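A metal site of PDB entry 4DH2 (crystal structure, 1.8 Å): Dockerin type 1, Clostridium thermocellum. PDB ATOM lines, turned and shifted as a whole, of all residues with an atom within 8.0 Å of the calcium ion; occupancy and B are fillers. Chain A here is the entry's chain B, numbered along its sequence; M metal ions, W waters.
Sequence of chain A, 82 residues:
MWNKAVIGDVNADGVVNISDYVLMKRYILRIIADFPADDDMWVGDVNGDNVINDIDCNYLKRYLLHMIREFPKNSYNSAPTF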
ATOM      1  N   VAL A   6       5.434   9.251  13.274  1.00  0.00           N
ATOM      2  CA  VAL A   6       6.432   8.578  12.466  1.00  0.00           C
ATOM      3  C   VAL A   6       7.758   9.322  12.469  1.00  0.00           C
ATOM      4  O   VAL A   6       7.801  10.525  12.192  1.00  0.00           O
ATOM      5  CB  VAL A   6       5.961   8.381  10.998  1.00  0.00           C
ATOM      6  CG1 VAL A   6       7.066   7.742  10.182  1.00  0.00           C
ATOM      7  CG2 VAL A   6       4.669   7.536  10.951  1.00  0.00           C
ATOM      8  N   GLY A   8      11.034  10.857  11.314  1.00  0.00           N
ATOM      9  CA  GLY A   8      11.420  11.376  10.009  1.00  0.00           C
ATOM     10  C   GLY A   8      10.257  12.073   9.347  1.00  0.00           C
ATOM     11  O   GLY A   8      10.458  12.797   8.378  1.00  0.00           O
ATOM     12  N   ASP A   9       9.038  11.891   9.877  1.00  0.00           N
ATOM     13  CA  ASP A   9       7.851  12.445   9.231  1.00  0.00           C
ATOM     14  C   ASP A   9       7.533  13.814   9.835  1.00  0.00           C
ATOM     15  O   ASP A   9       6.649  13.965  10.698  1.00  0.00           O
ATOM     16  CB  ASP A   9       6.651  11.490   9.371  1.00  0.00           C
ATOM     17  CG  ASP A   9       5.389  12.054   8.774  1.00  0.00           C
ATOM     18  OD1 ASP A   9       5.470  12.986   7.959  1.00  0.00           O
ATOM     19  OD2 ASP A   9       4.281  11.589   9.141  1.00  0.00           O
ATOM     20  N   VAL A  10       8.286  14.814   9.394  1.00  0.00           N
ATOM     21  CA  VAL A  10       8.248  16.097  10.041  1.00  0.00           C
ATOM     22  C   VAL A  10       7.068  16.971   9.648  1.00  0.00           C
ATOM     23  O   VAL A  10       6.847  17.983  10.291  1.00  0.00           O
ATOM     24  CB  VAL A  10       9.584  16.877   9.847  1.00  0.00           C
ATOM     25  CG1 VAL A  10      10.762  16.044  10.377  1.00  0.00           C
ATOM     26  CG2 VAL A  10       9.779  17.287   8.409  1.00  0.00           C
ATOM     27  N   ASN A  11       6.292  16.586   8.631  1.00  0.00           N
ATOM     28  CA  ASN A  11       5.038  17.304   8.346  1.00  0.00           C
ATOM     29  C   ASN A  11       3.808  16.486   8.727  1.00  0.00           C
ATOM     30  O   ASN A  11       2.697  16.887   8.425  1.00  0.00           O
ATOM     31  CB  ASN A  11       4.935  17.756   6.887  1.00  0.00           C
ATOM     32  CG  ASN A  11       5.058  16.621   5.880  1.00  0.00           C
ATOM     33  OD1 ASN A  11       5.077  15.430   6.209  1.00  0.00           O
ATOM     34  ND2 ASN A  11       5.147  17.018   4.613  1.00  0.00           N
ATOM     35  N   ALA A  12       4.033  15.350   9.386  1.00  0.00           N
ATOM     36  CA  ALA A  12       2.963  14.534   9.946  1.00  0.00           C
ATOM     37  C   ALA A  12       1.925  14.149   8.888  1.00  0.00           C
ATOM     38  O   ALA A  12       0.717  14.246   9.125  1.00  0.00           O
ATOM     39  CB  ALA A  12       2.291  15.270  11.152  1.00  0.00           C
ATOM     40  N   ASP A  13       2.381  13.717   7.719  1.00  0.00           N
ATOM     41  CA  ASP A  13       1.428  13.320   6.689  1.00  0.00           C
ATOM     42  C   ASP A  13       1.444  11.801   6.531  1.00  0.00           C
ATOM     43  O   ASP A  13       0.840  11.270   5.617  1.00  0.00           O
ATOM     44  CB  ASP A  13       1.669  14.055   5.357  1.00  0.00           C
ATOM     45  CG  ASP A  13       2.950  13.613   4.658  1.00  0.00           C
ATOM     46  OD1 ASP A  13       3.732  12.838   5.236  1.00  0.00           O
ATOM     47  OD2 ASP A  13       3.163  14.048   3.499  1.00  0.00           O
ATOM     48  N   GLY A  14       2.128  11.118   7.444  1.00  0.00           N
ATOM     49  CA  GLY A  14       2.117   9.662   7.448  1.00  0.00           C
ATOM     50  C   GLY A  14       3.293   8.982   6.784  1.00  0.00           C
ATOM     51  O   GLY A  14       3.504   7.779   6.988  1.00  0.00           O
ATOM     52  N   VAL A  15       4.066   9.715   5.989  1.00  0.00           N
ATOM     53  CA  VAL A  15       5.106   9.116   5.172  1.00  0.00           C
ATOM     54  C   VAL A  15       6.371   9.986   5.214  1.00  0.00           C
ATOM     55  O   VAL A  15       6.275  11.173   5.510  1.00  0.00           O
ATOM     56  CB  VAL A  15       4.655   8.971   3.692  1.00  0.00           C
ATOM     57  CG1 VAL A  15       4.350  10.318   3.108  1.00  0.00           C
ATOM     58  CG2 VAL A  15       5.721   8.260   2.872  1.00  0.00           C
ATOM     59  N   VAL A  16       7.511   9.361   4.960  1.00  0.00           N
ATOM     60  CA  VAL A  16       8.775  10.072   4.883  1.00  0.00           C
ATOM     61  C   VAL A  16       9.167  10.163   3.415  1.00  0.00           C
ATOM     62  O   VAL A  16       9.425   9.135   2.768  1.00  0.00           O
ATOM     63  CB  VAL A  16       9.852   9.338   5.675  1.00  0.00           C
ATOM     64  CG1 VAL A  16      11.166  10.063   5.574  1.00  0.00           C
ATOM     65  CG2 VAL A  16       9.388   9.221   7.145  1.00  0.00           C
ATOM     66  N   ASN A  17       9.193  11.383   2.879  1.00  0.00           N
ATOM     67  CA  ASN A  17       9.542  11.572   1.490  1.00  0.00           C
ATOM     68  C   ASN A  17      10.251  12.923   1.317  1.00  0.00           C
ATOM     69  O   ASN A  17      10.678  13.543   2.313  1.00  0.00           O
ATOM     70  CB  ASN A  17       8.307  11.466   0.563  1.00  0.00           C
ATOM     71  CG  ASN A  17       7.252  12.516   0.846  1.00  0.00           C
ATOM     72  OD1 ASN A  17       7.525  13.536   1.462  1.00  0.00           O
ATOM     73  ND2 ASN A  17       5.996  12.244   0.413  1.00  0.00           N
ATOM     74  N   ILE A  18      10.404  13.346   0.069  1.00  0.00           N
ATOM     75  CA  ILE A  18      11.185  14.542  -0.186  1.00  0.00           C
ATOM     76  C   ILE A  18      10.668  15.761   0.578  1.00  0.00           C
ATOM     77  O   ILE A  18      11.444  16.630   0.925  1.00  0.00           O
ATOM     78  CB  ILE A  18      11.224  14.919  -1.691  1.00  0.00           C
ATOM     79  CG1 ILE A  18       9.803  15.020  -2.246  1.00  0.00           C
ATOM     80  CG2 ILE A  18      12.069  13.899  -2.445  1.00  0.00           C
ATOM     81  CD1 ILE A  18       9.710  15.520  -3.615  1.00  0.00           C
ATOM     82  N   SER A  19       9.356  15.860   0.819  1.00  0.00           N
ATOM     83  CA  SER A  19       8.899  17.032   1.544  1.00  0.00           C
ATOM     84  C   SER A  19       9.523  17.113   2.941  1.00  0.00           C
ATOM     85  O   SER A  19       9.811  18.212   3.447  1.00  0.00           O
ATOM     86  CB  SER A  19       7.361  17.089   1.619  1.00  0.00           C
ATOM     87  OG  SER A  19       6.823  17.276   0.320  1.00  0.00           O
ATOM     88  N   ASP A  20       9.676  15.969   3.606  1.00  0.00           N
ATOM     89  CA  ASP A  20      10.289  15.966   4.917  1.00  0.00           C
ATOM     90  C   ASP A  20      11.754  16.356   4.841  1.00  0.00           C
ATOM     91  O   ASP A  20      12.294  17.010   5.740  1.00  0.00           O
ATOM     92  CB  ASP A  20      10.164  14.602   5.537  1.00  0.00           C
ATOM     93  CG  ASP A  20       8.708  14.177   5.651  1.00  0.00           C
ATOM     94  OD1 ASP A  20       7.974  14.749   6.472  1.00  0.00           O
ATOM     95  OD2 ASP A  20       8.312  13.316   4.840  1.00  0.00           O
ATOM     96  N   TYR A  21      12.413  15.943   3.767  1.00  0.00           N
ATOM     97  CA  TYR A  21      13.811  16.305   3.551  1.00  0.00           C
ATOM     98  C   TYR A  21      13.982  17.816   3.353  1.00  0.00           C
ATOM     99  O   TYR A  21      14.864  18.461   3.955  1.00  0.00           O
ATOM    100  CB  TYR A  21      14.333  15.560   2.322  1.00  0.00           C
ATOM    101  CG  TYR A  21      15.806  15.697   2.035  1.00  0.00           C
ATOM    102  CD1 TYR A  21      16.757  15.368   2.984  1.00  0.00           C
ATOM    103  CD2 TYR A  21      16.251  16.120   0.781  1.00  0.00           C
ATOM    104  CE1 TYR A  21      18.097  15.485   2.719  1.00  0.00           C
ATOM    105  CE2 TYR A  21      17.604  16.238   0.512  1.00  0.00           C
ATOM    106  CZ  TYR A  21      18.515  15.910   1.498  1.00  0.00           C
ATOM    107  OH  TYR A  21      19.863  16.021   1.255  1.00  0.00           O
ATOM    108  N   LEU A  23      11.866  20.156   4.245  1.00  0.00           N
ATOM    109  CA  LEU A  23      11.525  20.798   5.508  1.00  0.00           C
ATOM    110  C   LEU A  23      12.668  20.716   6.546  1.00  0.00           C
ATOM    111  O   LEU A  23      12.967  21.708   7.248  1.00  0.00           O
ATOM    112  CB  LEU A  23      10.234  20.222   6.095  1.00  0.00           C
ATOM    113  CG  LEU A  23       8.947  20.644   5.379  1.00  0.00           C
ATOM    114  CD1 LEU A  23       7.791  19.807   5.902  1.00  0.00           C
ATOM    115  CD2 LEU A  23       8.633  22.125   5.530  1.00  0.00           C
HETATM  116 CA    CA M   1       6.054  13.429   5.678  1.00  0.00          CA
HETATM  117  O   HOH W   1       5.800  14.248   3.421  1.00  0.00           O
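The side-chain carboxylate of Asp 9 sits close to the backbone NH of Ala 12 (3.1 Å).
N of Gly 14 is in hydrogen-bond range of OD2 of Asp 9 (2.8 Å).
OD1 of Asp 20 lies close to N of Val 10 (2.9 Å).
OD2 of Asp 20 lies close to N of Asn 17 (2.9 Å).
Five residues have an atom within 4 Å of the calcium ion: Asp 9, Asn 11, Asp 13, Val 15 and Asp 20.
The nearest printed residue that does not touch the calcium ion is Val 16 (4.4 Å).
The calcium ion is bound by the backbone carbonyl oxygen (O) of Val 15 (2.3 Å), the side-chain amide oxygen (OD1) of Asn 11 (2.3 Å), the side-chain carboxylate (OD1) of Asp 9 (2.4 Å), the side-chain carboxylate (OD2) of Asp 20 (2.4 Å), water W1 (2.4 Å), the side-chain carboxylate (OD1) of Asp 13 (2.4 Å) and the side-chain carboxylate (OD1) of Asp 20 (2.5 Å).
The calcium ion has seven donor atoms within binding distance.
Water W1 lies within hydrogen-bond range of OD2 of Asp 13 (2.6 Å), OD1 of Asn 17 (2.7 Å) and ND2 of Asn 11 (3.1 Å).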
